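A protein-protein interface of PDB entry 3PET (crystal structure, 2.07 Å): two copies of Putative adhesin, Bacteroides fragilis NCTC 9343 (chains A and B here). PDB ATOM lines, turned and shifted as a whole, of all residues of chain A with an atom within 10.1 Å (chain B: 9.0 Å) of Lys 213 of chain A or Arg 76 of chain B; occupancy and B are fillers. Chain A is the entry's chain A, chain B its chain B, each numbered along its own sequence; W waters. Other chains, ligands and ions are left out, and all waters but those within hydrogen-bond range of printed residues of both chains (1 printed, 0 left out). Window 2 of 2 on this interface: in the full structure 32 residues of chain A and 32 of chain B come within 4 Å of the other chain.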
ATOM      1  N   SER A 174      14.764   4.314 -28.509  1.00  0.00           N
ATOM      2  CA  SER A 174      15.776   5.228 -27.989  1.00  0.00           C
ATOM      3  C   SER A 174      15.084   6.309 -27.186  1.00  0.00           C
ATOM      4  O   SER A 174      14.116   6.894 -27.663  1.00  0.00           O
ATOM      5  CB  SER A 174      16.650   5.804 -29.100  1.00  0.00           C
ATOM      6  OG  SER A 174      17.536   6.784 -28.586  1.00  0.00           O
ATOM      7  N   SER A 175      15.535   6.493 -25.915  1.00  0.00           N
ATOM      8  CA  SER A 175      14.969   7.470 -24.992  1.00  0.00           C
ATOM      9  C   SER A 175      16.015   8.574 -24.762  1.00  0.00           C
ATOM     10  O   SER A 175      17.075   8.280 -24.202  1.00  0.00           O
ATOM     11  CB  SER A 175      14.537   6.775 -23.693  1.00  0.00           C
ATOM     12  OG  SER A 175      15.633   6.127 -23.060  1.00  0.00           O
ATOM     13  N   GLN A 176      15.757   9.818 -25.261  1.00  0.00           N
ATOM     14  CA  GLN A 176      16.711  10.945 -25.201  1.00  0.00           C
ATOM     15  C   GLN A 176      16.202  12.166 -24.421  1.00  0.00           C
ATOM     16  O   GLN A 176      16.983  13.080 -24.151  1.00  0.00           O
ATOM     17  CB  GLN A 176      17.083  11.408 -26.611  1.00  0.00           C
ATOM     18  CG  GLN A 176      17.853  10.402 -27.433  1.00  0.00           C
ATOM     19  CD  GLN A 176      18.042  10.939 -28.831  1.00  0.00           C
ATOM     20  OE1 GLN A 176      17.163  10.841 -29.666  1.00  0.00           O
ATOM     21  NE2 GLN A 176      19.157  11.618 -29.078  1.00  0.00           N
ATOM     22  N   GLY A 177      14.915  12.175 -24.071  1.00  0.00           N
ATOM     23  CA  GLY A 177      14.345  13.260 -23.276  1.00  0.00           C
ATOM     24  C   GLY A 177      14.123  12.808 -21.849  1.00  0.00           C
ATOM     25  O   GLY A 177      14.929  12.051 -21.284  1.00  0.00           O
ATOM     26  N   ALA A 191      17.762  -1.283 -28.007  1.00  0.00           N
ATOM     27  CA  ALA A 191      17.310  -0.282 -27.035  1.00  0.00           C
ATOM     28  C   ALA A 191      18.467   0.570 -26.552  1.00  0.00           C
ATOM     29  O   ALA A 191      19.537   0.027 -26.231  1.00  0.00           O
ATOM     30  CB  ALA A 191      16.618  -0.966 -25.845  1.00  0.00           C
ATOM     31  N   ALA A 192      18.269   1.919 -26.525  1.00  0.00           N
ATOM     32  CA  ALA A 192      19.322   2.839 -26.082  1.00  0.00           C
ATOM     33  C   ALA A 192      18.777   3.881 -25.114  1.00  0.00           C
ATOM     34  O   ALA A 192      17.969   4.715 -25.513  1.00  0.00           O
ATOM     35  CB  ALA A 192      19.958   3.527 -27.289  1.00  0.00           C
ATOM     36  N   VAL A 193      19.274   3.881 -23.850  1.00  0.00           N
ATOM     37  CA  VAL A 193      18.879   4.881 -22.829  1.00  0.00           C
ATOM     38  C   VAL A 193      19.870   6.045 -22.925  1.00  0.00           C
ATOM     39  O   VAL A 193      21.071   5.841 -22.750  1.00  0.00           O
ATOM     40  CB  VAL A 193      18.784   4.269 -21.395  1.00  0.00           C
ATOM     41  CG1 VAL A 193      18.925   5.335 -20.298  1.00  0.00           C
ATOM     42  CG2 VAL A 193      17.477   3.502 -21.226  1.00  0.00           C
ATOM     43  N   ARG A 194      19.385   7.247 -23.270  1.00  0.00           N
ATOM     44  CA  ARG A 194      20.270   8.412 -23.456  1.00  0.00           C
ATOM     45  C   ARG A 194      19.780   9.678 -22.736  1.00  0.00           C
ATOM     46  O   ARG A 194      20.438  10.711 -22.825  1.00  0.00           O
ATOM     47  CB  ARG A 194      20.430   8.733 -24.958  1.00  0.00           C
ATOM     48  CG  ARG A 194      21.098   7.659 -25.834  1.00  0.00           C
ATOM     49  CD  ARG A 194      22.604   7.608 -25.599  1.00  0.00           C
ATOM     50  NE  ARG A 194      23.305   6.786 -26.593  1.00  0.00           N
ATOM     51  CZ  ARG A 194      23.486   5.469 -26.502  1.00  0.00           C
ATOM     52  NH1 ARG A 194      23.010   4.795 -25.458  1.00  0.00           N
ATOM     53  NH2 ARG A 194      24.143   4.817 -27.453  1.00  0.00           N
ATOM     54  N   GLY A 195      18.674   9.583 -21.992  1.00  0.00           N
ATOM     55  CA  GLY A 195      18.162  10.726 -21.236  1.00  0.00           C
ATOM     56  C   GLY A 195      17.898  10.367 -19.795  1.00  0.00           C
ATOM     57  O   GLY A 195      18.668   9.617 -19.186  1.00  0.00           O
ATOM     58  N   VAL A 196      16.785  10.885 -19.244  1.00  0.00           N
ATOM     59  CA  VAL A 196      16.348  10.572 -17.883  1.00  0.00           C
ATOM     60  C   VAL A 196      15.095   9.735 -18.033  1.00  0.00           C
ATOM     61  O   VAL A 196      14.033  10.246 -18.387  1.00  0.00           O
ATOM     62  CB  VAL A 196      16.140  11.822 -16.990  1.00  0.00           C
ATOM     63  CG1 VAL A 196      15.765  11.415 -15.567  1.00  0.00           C
ATOM     64  CG2 VAL A 196      17.393  12.691 -16.959  1.00  0.00           C
ATOM     65  N   GLY A 197      15.237   8.442 -17.821  1.00  0.00           N
ATOM     66  CA  GLY A 197      14.121   7.524 -17.992  1.00  0.00           C
ATOM     67  C   GLY A 197      14.619   6.180 -18.460  1.00  0.00           C
ATOM     68  O   GLY A 197      15.789   6.033 -18.851  1.00  0.00           O
ATOM     69  N   SER A 198      13.720   5.206 -18.433  1.00  0.00           N
ATOM     70  CA  SER A 198      14.017   3.810 -18.692  1.00  0.00           C
ATOM     71  C   SER A 198      13.280   3.212 -19.859  1.00  0.00           C
ATOM     72  O   SER A 198      12.227   3.705 -20.248  1.00  0.00           O
ATOM     73  CB  SER A 198      13.671   2.996 -17.449  1.00  0.00           C
ATOM     74  OG  SER A 198      14.408   3.491 -16.343  1.00  0.00           O
ATOM     75  N   ILE A 199      13.816   2.100 -20.382  1.00  0.00           N
ATOM     76  CA  ILE A 199      13.166   1.320 -21.451  1.00  0.00           C
ATOM     77  C   ILE A 199      12.795  -0.048 -20.866  1.00  0.00           C
ATOM     78  O   ILE A 199      13.654  -0.766 -20.354  1.00  0.00           O
ATOM     79  CB  ILE A 199      14.020   1.208 -22.749  1.00  0.00           C
ATOM     80  CG1 ILE A 199      14.300   2.623 -23.343  1.00  0.00           C
ATOM     81  CG2 ILE A 199      13.341   0.277 -23.770  1.00  0.00           C
ATOM     82  CD1 ILE A 199      15.347   2.705 -24.438  1.00  0.00           C
ATOM     83  N   SER A 209      20.185  -5.743 -28.426  1.00  0.00           N
ATOM     84  CA  SER A 209      21.324  -4.824 -28.391  1.00  0.00           C
ATOM     85  C   SER A 209      20.932  -3.697 -27.455  1.00  0.00           C
ATOM     86  O   SER A 209      19.984  -2.968 -27.740  1.00  0.00           O
ATOM     87  CB  SER A 209      21.664  -4.321 -29.790  1.00  0.00           C
ATOM     88  OG  SER A 209      22.915  -3.657 -29.724  1.00  0.00           O
ATOM     89  N   LEU A 210      21.563  -3.653 -26.279  1.00  0.00           N
ATOM     90  CA  LEU A 210      21.209  -2.709 -25.240  1.00  0.00           C
ATOM     91  C   LEU A 210      22.375  -1.774 -24.894  1.00  0.00           C
ATOM     92  O   LEU A 210      23.523  -2.209 -24.753  1.00  0.00           O
ATOM     93  CB  LEU A 210      20.725  -3.451 -23.981  1.00  0.00           C
ATOM     94  CG  LEU A 210      19.768  -4.642 -24.185  1.00  0.00           C
ATOM     95  CD1 LEU A 210      19.559  -5.422 -22.864  1.00  0.00           C
ATOM     96  CD2 LEU A 210      18.452  -4.219 -24.832  1.00  0.00           C
ATOM     97  N   SER A 211      22.051  -0.479 -24.744  1.00  0.00           N
ATOM     98  CA  SER A 211      23.015   0.573 -24.458  1.00  0.00           C
ATOM     99  C   SER A 211      22.453   1.474 -23.382  1.00  0.00           C
ATOM    100  O   SER A 211      21.388   2.048 -23.558  1.00  0.00           O
ATOM    101  CB  SER A 211      23.305   1.364 -25.735  1.00  0.00           C
ATOM    102  OG  SER A 211      24.258   2.384 -25.503  1.00  0.00           O
ATOM    103  N   LYS A 212      23.164   1.601 -22.266  1.00  0.00           N
ATOM    104  CA  LYS A 212      22.739   2.438 -21.141  1.00  0.00           C
ATOM    105  C   LYS A 212      23.694   3.616 -21.031  1.00  0.00           C
ATOM    106  O   LYS A 212      24.813   3.447 -20.558  1.00  0.00           O
ATOM    107  CB  LYS A 212      22.726   1.604 -19.843  1.00  0.00           C
ATOM    108  CG  LYS A 212      21.615   0.558 -19.793  1.00  0.00           C
ATOM    109  CD  LYS A 212      21.631  -0.202 -18.475  1.00  0.00           C
ATOM    110  N   LYS A 213      23.285   4.802 -21.493  1.00  0.00           N
ATOM    111  CA  LYS A 213      24.177   5.967 -21.460  1.00  0.00           C
ATOM    112  C   LYS A 213      23.467   7.235 -20.943  1.00  0.00           C
ATOM    113  O   LYS A 213      23.755   8.341 -21.410  1.00  0.00           O
ATOM    114  CB  LYS A 213      24.794   6.181 -22.860  1.00  0.00           C
ATOM    115  CG  LYS A 213      25.939   5.195 -23.137  1.00  0.00           C
ATOM    116  CD  LYS A 213      26.389   5.188 -24.581  1.00  0.00           C
ATOM    117  CE  LYS A 213      27.743   4.539 -24.759  1.00  0.00           C
ATOM    118  NZ  LYS A 213      27.643   3.072 -24.978  1.00  0.00           N
ATOM    119  N   GLY A 214      22.598   7.060 -19.942  1.00  0.00           N
ATOM    120  CA  GLY A 214      21.809   8.131 -19.328  1.00  0.00           C
ATOM    121  C   GLY A 214      21.495   7.842 -17.880  1.00  0.00           C
ATOM    122  O   GLY A 214      22.293   7.196 -17.191  1.00  0.00           O
ATOM    123  N   VAL A 215      20.334   8.302 -17.410  1.00  0.00           N
ATOM    124  CA  VAL A 215      19.886   8.064 -16.026  1.00  0.00           C
ATOM    125  C   VAL A 215      18.638   7.220 -16.135  1.00  0.00           C
ATOM    126  O   VAL A 215      17.570   7.730 -16.458  1.00  0.00           O
ATOM    127  CB  VAL A 215      19.683   9.396 -15.218  1.00  0.00           C
ATOM    128  CG1 VAL A 215      19.303   9.116 -13.765  1.00  0.00           C
ATOM    129  CG2 VAL A 215      20.930  10.267 -15.279  1.00  0.00           C
ATOM    130  N   GLY A 216      18.813   5.927 -15.967  1.00  0.00           N
ATOM    131  CA  GLY A 216      17.738   4.962 -16.097  1.00  0.00           C
ATOM    132  C   GLY A 216      18.265   3.617 -16.546  1.00  0.00           C
ATOM    133  O   GLY A 216      19.452   3.455 -16.808  1.00  0.00           O
ATOM    134  N   THR A 217      17.382   2.664 -16.710  1.00  0.00           N
ATOM    135  CA  THR A 217      17.830   1.328 -17.086  1.00  0.00           C
ATOM    136  C   THR A 217      16.999   0.710 -18.218  1.00  0.00           C
ATOM    137  O   THR A 217      16.050   1.322 -18.712  1.00  0.00           O
ATOM    138  CB  THR A 217      17.802   0.438 -15.836  1.00  0.00           C
ATOM    139  OG1 THR A 217      18.536  -0.751 -16.122  1.00  0.00           O
ATOM    140  CG2 THR A 217      16.364   0.113 -15.374  1.00  0.00           C
ATOM    141  N   ILE A 218      17.407  -0.500 -18.639  1.00  0.00           N
ATOM    142  CA  ILE A 218      16.732  -1.306 -19.656  1.00  0.00           C
ATOM    143  C   ILE A 218      16.363  -2.586 -18.934  1.00  0.00           C
ATOM    144  O   ILE A 218      17.230  -3.239 -18.355  1.00  0.00           O
ATOM    145  CB  ILE A 218      17.584  -1.536 -20.940  1.00  0.00           C
ATOM    146  CG1 ILE A 218      17.993  -0.184 -21.578  1.00  0.00           C
ATOM    147  CG2 ILE A 218      16.824  -2.435 -21.944  1.00  0.00           C
ATOM    148  CD1 ILE A 218      19.046  -0.259 -22.625  1.00  0.00           C
ATOM    149  N   GLY B   4      36.424   0.869 -24.579  1.00  0.00           N
ATOM    150  CA  GLY B   4      35.426   1.495 -23.717  1.00  0.00           C
ATOM    151  C   GLY B   4      35.556   1.040 -22.278  1.00  0.00           C
ATOM    152  O   GLY B   4      35.927  -0.113 -22.032  1.00  0.00           O
ATOM    153  N   ILE B   5      35.258   1.933 -21.313  1.00  0.00           N
ATOM    154  CA  ILE B   5      35.393   1.583 -19.894  1.00  0.00           C
ATOM    155  C   ILE B   5      34.165   0.775 -19.405  1.00  0.00           C
ATOM    156  O   ILE B   5      33.021   1.194 -19.584  1.00  0.00           O
ATOM    157  CB  ILE B   5      35.662   2.841 -19.000  1.00  0.00           C
ATOM    158  CG1 ILE B   5      37.007   3.506 -19.370  1.00  0.00           C
ATOM    159  CG2 ILE B   5      35.659   2.479 -17.513  1.00  0.00           C
ATOM    160  CD1 ILE B   5      37.286   4.869 -18.718  1.00  0.00           C
ATOM    161  N   GLN B   6      34.421  -0.373 -18.773  1.00  0.00           N
ATOM    162  CA  GLN B   6      33.362  -1.184 -18.190  1.00  0.00           C
ATOM    163  C   GLN B   6      33.176  -0.725 -16.745  1.00  0.00           C
ATOM    164  O   GLN B   6      34.152  -0.768 -15.987  1.00  0.00           O
ATOM    165  CB  GLN B   6      33.698  -2.692 -18.266  1.00  0.00           C
ATOM    166  CG  GLN B   6      32.820  -3.516 -19.225  1.00  0.00           C
ATOM    167  CD  GLN B   6      31.322  -3.474 -18.959  1.00  0.00           C
ATOM    168  OE1 GLN B   6      30.825  -3.826 -17.881  1.00  0.00           O
ATOM    169  NE2 GLN B   6      30.564  -3.093 -19.980  1.00  0.00           N
ATOM    170  N   PRO B   7      31.978  -0.235 -16.335  1.00  0.00           N
ATOM    171  CA  PRO B   7      31.806   0.187 -14.923  1.00  0.00           C
ATOM    172  C   PRO B   7      32.090  -0.965 -13.961  1.00  0.00           C
ATOM    173  O   PRO B   7      31.645  -2.098 -14.212  1.00  0.00           O
ATOM    174  CB  PRO B   7      30.339   0.624 -14.848  1.00  0.00           C
ATOM    175  CG  PRO B   7      29.682  -0.055 -16.011  1.00  0.00           C
ATOM    176  CD  PRO B   7      30.720  -0.096 -17.098  1.00  0.00           C
ATOM    177  N   THR B  28      27.561  16.758 -15.910  1.00  0.00           N
ATOM    178  CA  THR B  28      27.674  15.338 -15.579  1.00  0.00           C
ATOM    179  C   THR B  28      26.407  14.532 -15.901  1.00  0.00           C
ATOM    180  O   THR B  28      25.342  15.096 -16.206  1.00  0.00           O
ATOM    181  CB  THR B  28      28.027  15.177 -14.062  1.00  0.00           C
ATOM    182  OG1 THR B  28      27.247  16.102 -13.298  1.00  0.00           O
ATOM    183  CG2 THR B  28      29.483  15.439 -13.780  1.00  0.00           C
ATOM    184  N   VAL B  29      26.548  13.187 -15.847  1.00  0.00           N
ATOM    185  CA  VAL B  29      25.444  12.263 -16.018  1.00  0.00           C
ATOM    186  C   VAL B  29      25.114  11.747 -14.618  1.00  0.00           C
ATOM    187  O   VAL B  29      25.985  11.195 -13.939  1.00  0.00           O
ATOM    188  CB  VAL B  29      25.727  11.116 -17.023  1.00  0.00           C
ATOM    189  CG1 VAL B  29      24.548  10.148 -17.084  1.00  0.00           C
ATOM    190  CG2 VAL B  29      26.047  11.661 -18.410  1.00  0.00           C
ATOM    191  N   GLY B  30      23.873  11.954 -14.190  1.00  0.00           N
ATOM    192  CA  GLY B  30      23.456  11.533 -12.857  1.00  0.00           C
ATOM    193  C   GLY B  30      22.602  12.574 -12.168  1.00  0.00           C
ATOM    194  O   GLY B  30      22.723  13.775 -12.456  1.00  0.00           O
ATOM    195  N   ASN B  51      35.408   3.475 -10.976  1.00  0.00           N
ATOM    196  CA  ASN B  51      36.110   3.890 -12.199  1.00  0.00           C
ATOM    197  C   ASN B  51      35.296   4.905 -13.010  1.00  0.00           C
ATOM    198  O   ASN B  51      35.844   5.543 -13.909  1.00  0.00           O
ATOM    199  CB  ASN B  51      36.484   2.674 -13.061  1.00  0.00           C
ATOM    200  CG  ASN B  51      35.324   1.818 -13.500  1.00  0.00           C
ATOM    201  OD1 ASN B  51      34.217   1.869 -12.952  1.00  0.00           O
ATOM    202  ND2 ASN B  51      35.571   0.972 -14.475  1.00  0.00           N
ATOM    203  N   ILE B  52      33.997   5.050 -12.706  1.00  0.00           N
ATOM    204  CA  ILE B  52      33.120   6.019 -13.383  1.00  0.00           C
ATOM    205  C   ILE B  52      33.159   7.307 -12.563  1.00  0.00           C
ATOM    206  O   ILE B  52      33.309   8.377 -13.136  1.00  0.00           O
ATOM    207  CB  ILE B  52      31.687   5.470 -13.615  1.00  0.00           C
ATOM    208  CG1 ILE B  52      31.695   4.076 -14.311  1.00  0.00           C
ATOM    209  CG2 ILE B  52      30.796   6.476 -14.364  1.00  0.00           C
ATOM    210  CD1 ILE B  52      32.546   3.907 -15.659  1.00  0.00           C
ATOM    211  N   LEU B  55      36.013   9.594 -13.342  1.00  0.00           N
ATOM    212  CA  LEU B  55      35.917  10.383 -14.581  1.00  0.00           C
ATOM    213  C   LEU B  55      35.351  11.787 -14.363  1.00  0.00           C
ATOM    214  O   LEU B  55      35.351  12.584 -15.302  1.00  0.00           O
ATOM    215  CB  LEU B  55      35.041   9.686 -15.634  1.00  0.00           C
ATOM    216  CG  LEU B  55      35.428   8.274 -16.076  1.00  0.00           C
ATOM    217  CD1 LEU B  55      34.436   7.763 -17.066  1.00  0.00           C
ATOM    218  CD2 LEU B  55      36.832   8.225 -16.682  1.00  0.00           C
ATOM    219  N   ILE B  69      32.583  15.936 -17.153  1.00  0.00           N
ATOM    220  CA  ILE B  69      33.048  14.587 -17.475  1.00  0.00           C
ATOM    221  C   ILE B  69      34.281  14.663 -18.351  1.00  0.00           C
ATOM    222  O   ILE B  69      34.313  15.451 -19.306  1.00  0.00           O
ATOM    223  CB  ILE B  69      31.962  13.708 -18.174  1.00  0.00           C
ATOM    224  CG1 ILE B  69      30.556  13.875 -17.560  1.00  0.00           C
ATOM    225  CG2 ILE B  69      32.384  12.224 -18.218  1.00  0.00           C
ATOM    226  CD1 ILE B  69      29.440  13.501 -18.490  1.00  0.00           C
ATOM    227  N   LYS B  73      37.709   9.459 -22.389  1.00  0.00           N
ATOM    228  CA  LYS B  73      37.587   8.046 -22.088  1.00  0.00           C
ATOM    229  C   LYS B  73      36.135   7.597 -22.302  1.00  0.00           C
ATOM    230  O   LYS B  73      35.243   7.998 -21.552  1.00  0.00           O
ATOM    231  CB  LYS B  73      38.067   7.769 -20.657  1.00  0.00           C
ATOM    232  N   LYS B  74      35.905   6.816 -23.374  1.00  0.00           N
ATOM    233  CA  LYS B  74      34.616   6.220 -23.737  1.00  0.00           C
ATOM    234  C   LYS B  74      34.140   5.287 -22.628  1.00  0.00           C
ATOM    235  O   LYS B  74      34.964   4.615 -22.005  1.00  0.00           O
ATOM    236  CB  LYS B  74      34.754   5.439 -25.054  1.00  0.00           C
ATOM    237  N   VAL B  75      32.829   5.281 -22.353  1.00  0.00           N
ATOM    238  CA  VAL B  75      32.215   4.465 -21.304  1.00  0.00           C
ATOM    239  C   VAL B  75      31.154   3.579 -21.951  1.00  0.00           C
ATOM    240  O   VAL B  75      30.318   4.084 -22.698  1.00  0.00           O
ATOM    241  CB  VAL B  75      31.637   5.361 -20.174  1.00  0.00           C
ATOM    242  CG1 VAL B  75      30.981   4.540 -19.060  1.00  0.00           C
ATOM    243  CG2 VAL B  75      32.721   6.249 -19.593  1.00  0.00           C
ATOM    244  N   ARG B  76      31.202   2.257 -21.677  1.00  0.00           N
ATOM    245  CA  ARG B  76      30.274   1.280 -22.243  1.00  0.00           C
ATOM    246  C   ARG B  76      28.860   1.552 -21.802  1.00  0.00           C
ATOM    247  O   ARG B  76      27.979   1.845 -22.624  1.00  0.00           O
ATOM    248  CB  ARG B  76      30.676  -0.146 -21.826  1.00  0.00           C
ATOM    249  N   ASN B  77      28.629   1.384 -20.506  1.00  0.00           N
ATOM    250  CA  ASN B  77      27.328   1.544 -19.909  1.00  0.00           C
ATOM    251  C   ASN B  77      27.453   2.320 -18.628  1.00  0.00           C
ATOM    252  O   ASN B  77      28.444   2.208 -17.909  1.00  0.00           O
ATOM    253  CB  ASN B  77      26.659   0.175 -19.682  1.00  0.00           C
ATOM    254  CG  ASN B  77      26.266  -0.559 -20.965  1.00  0.00           C
ATOM    255  OD1 ASN B  77      25.701   0.008 -21.916  1.00  0.00           O
ATOM    256  ND2 ASN B  77      26.505  -1.860 -20.999  1.00  0.00           N
ATOM    257  N   PHE B  78      26.482   3.168 -18.388  1.00  0.00           N
ATOM    258  CA  PHE B  78      26.412   3.963 -17.181  1.00  0.00           C
ATOM    259  C   PHE B  78      25.628   3.176 -16.146  1.00  0.00           C
ATOM    260  O   PHE B  78      24.631   2.535 -16.482  1.00  0.00           O
ATOM    261  CB  PHE B  78      25.751   5.327 -17.469  1.00  0.00           C
ATOM    262  CG  PHE B  78      26.685   6.412 -17.956  1.00  0.00           C
ATOM    263  CD1 PHE B  78      27.354   7.236 -17.056  1.00  0.00           C
ATOM    264  CD2 PHE B  78      26.894   6.614 -19.317  1.00  0.00           C
ATOM    265  CE1 PHE B  78      28.206   8.254 -17.510  1.00  0.00           C
ATOM    266  CE2 PHE B  78      27.744   7.632 -19.771  1.00  0.00           C
ATOM    267  CZ  PHE B  78      28.396   8.446 -18.864  1.00  0.00           C
ATOM    268  N   LYS B  79      26.100   3.167 -14.912  1.00  0.00           N
ATOM    269  CA  LYS B  79      25.373   2.539 -13.815  1.00  0.00           C
ATOM    270  C   LYS B  79      24.778   3.682 -12.986  1.00  0.00           C
ATOM    271  O   LYS B  79      24.980   4.842 -13.348  1.00  0.00           O
ATOM    272  CB  LYS B  79      26.288   1.619 -12.985  1.00  0.00           C
ATOM    273  CG  LYS B  79      26.655   0.286 -13.624  1.00  0.00           C
ATOM    274  CD  LYS B  79      27.177  -0.646 -12.527  1.00  0.00           C
ATOM    275  CE  LYS B  79      28.005  -1.803 -13.018  1.00  0.00           C
ATOM    276  NZ  LYS B  79      28.630  -2.529 -11.879  1.00  0.00           N
ATOM    277  N   GLY B  97      24.080  18.763 -18.357  1.00  0.00           N
ATOM    278  CA  GLY B  97      24.329  17.329 -18.446  1.00  0.00           C
ATOM    279  C   GLY B  97      23.060  16.537 -18.655  1.00  0.00           C
ATOM    280  O   GLY B  97      22.132  17.006 -19.320  1.00  0.00           O
ATOM    281  N   VAL B  98      23.012  15.323 -18.077  1.00  0.00           N
ATOM    282  CA  VAL B  98      21.839  14.435 -18.163  1.00  0.00           C
ATOM    283  C   VAL B  98      21.505  14.038 -16.730  1.00  0.00           C
ATOM    284  O   VAL B  98      22.363  13.504 -16.038  1.00  0.00           O
ATOM    285  CB  VAL B  98      22.073  13.192 -19.100  1.00  0.00           C
ATOM    286  CG1 VAL B  98      20.881  12.244 -19.059  1.00  0.00           C
ATOM    287  CG2 VAL B  98      22.381  13.607 -20.535  1.00  0.00           C
ATOM    288  N   GLY B  99      20.305  14.360 -16.265  1.00  0.00           N
ATOM    289  CA  GLY B  99      19.936  14.022 -14.885  1.00  0.00           C
ATOM    290  C   GLY B  99      19.026  15.060 -14.271  1.00  0.00           C
ATOM    291  O   GLY B  99      18.915  16.172 -14.798  1.00  0.00           O
ATOM    292  N   VAL B 119      19.331  17.568 -20.268  1.00  0.00           N
ATOM    293  CA  VAL B 119      18.197  16.660 -20.279  1.00  0.00           C
ATOM    294  C   VAL B 119      17.917  16.298 -18.834  1.00  0.00           C
ATOM    295  O   VAL B 119      18.768  15.708 -18.171  1.00  0.00           O
ATOM    296  CB  VAL B 119      18.454  15.408 -21.175  1.00  0.00           C
ATOM    297  CG1 VAL B 119      17.263  14.455 -21.141  1.00  0.00           C
ATOM    298  CG2 VAL B 119      18.786  15.815 -22.609  1.00  0.00           C
HETATM  299  O   HOH W   1      23.895   7.216 -15.066  1.00  0.00           O
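The backbone carbonyl oxygen of Val 98 of chain B lies within hydrogen-bond range of the backbone NH of Gly 30 of chain B (2.8 Å).
The backbone NH of Arg 76 of chain B sits at hydrogen-bond distance from the backbone carbonyl oxygen of Ile 5 of chain B (3.0 Å).
N of Val 215 of chain A sits at hydrogen-bond distance from O of Gly 195 of chain A (2.8 Å).
The backbone carbonyl oxygen of Val 119 of chain B sits at hydrogen-bond distance from the backbone NH of Gly 99 of chain B.
The backbone carbonyl oxygen (O) of Val 193 of chain A lies within hydrogen-bond range of the backbone NH (N) of Gly 214 of chain A, 3.4 Å away.
N of Val 196 of chain A is in hydrogen-bond range of O of Gly 177 of chain A (3.0 Å).
The side-chain amino group of Lys 213 of chain A lies within hydrogen-bond range of the backbone carbonyl oxygen of Arg 76 of chain B, 2.7 Å away.
The backbone carbonyl oxygen of Lys 212 of chain A is in hydrogen-bond range of the backbone NH of Phe 78 of chain B (2.8 Å).
OD1 of Asn 77 of chain B sits at hydrogen-bond distance from N of Lys 212 of chain A (3.0 Å).
Hydrophobic or aromatic side chains of chain A within 4 Å of the printed part of chain B: Val 196 and Val 215.
Of the 22 printed residues of chain B, 9 touch a printed residue of chain A.
Printed residues of chain B that touch a printed residue of chain A: Val 29, Gly 30, Val 75, Arg 76, Asn 77, Phe 78, Val 98, Gly 99 and Val 119.
Among the printed residues, 17 pairs touch across the chains.
Printed residues of chain B within 4 Å of Ser 211 of chain A: Asn 77.
Printed residues of chain B within 4 Å of Lys 212 of chain A: Asn 77 (3.0 Å) and Phe 78 (2.8 Å).
Of chain B, only Val 75, Arg 76 and Phe 78 come within 4 Å of Lys 213 of chain A.
Gly 214 of chain A touches two residues of chain B.
Printed residues of chain B within 4 Å of Val 215 of chain A: Gly 30, Val 98 and Gly 99.
Of the printed residues of chain A, Gly 30 of chain B touches Val 215.
Val 75 of chain B touches just one residue of chain A: Lys 213 (3.3 Å).
Arg 76 of chain B touches one residue of chain A.
Printed residues of chain A within 4 Å of Asn 77 of chain B: Ser 211 (3.7 Å) and Lys 212 (3.0 Å).
The nearest printed residue of chain B that does not touch Val 215 of chain A is Val 29 of chain B (4.05 Å).
No position is printed for both chains.
Of the 17 pairs that touch across the chains among the printed residues, none has its exchanged pair printed and touching as well.
Water W1 bridges O of Gly 214 of chain A (2.7 Å) and O of Lys 79 of chain B (3.1 Å).
Among the printed residues, pairs that only touch across the chains: Gln 176 of chain A with Val 119 of chain B (3.3 Å), Lys 213 of chain A with Val 75 of chain B (3.3 Å), Gly 177 of chain A with Val 119 of chain B (3.4 Å), Val 196 of chain A with Gly 99 of chain B (3.4 Å), Gly 195 of chain A with Val 98 of chain B (3.4 Å), Lys 213 of chain A with Phe 78 of chain B (3.5 Å), Val 196 of chain A with Val 119 of chain B (3.5 Å), Val 215 of chain A with Gly 30 of chain B (3.6 Å), Val 215 of chain A with Val 98 of chain B (3.6 Å), Gly 214 of chain A with Val 29 of chain B (3.7 Å), Ser 211 of chain A with Asn 77 of chain B (3.7 Å), Gly 195 of chain A with Val 119 of chain B (3.8 Å), Val 215 of chain A with Gly 99 of chain B (3.9 Å) and Gly 214 of chain A with Phe 78 of chain B (3.9 Å).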
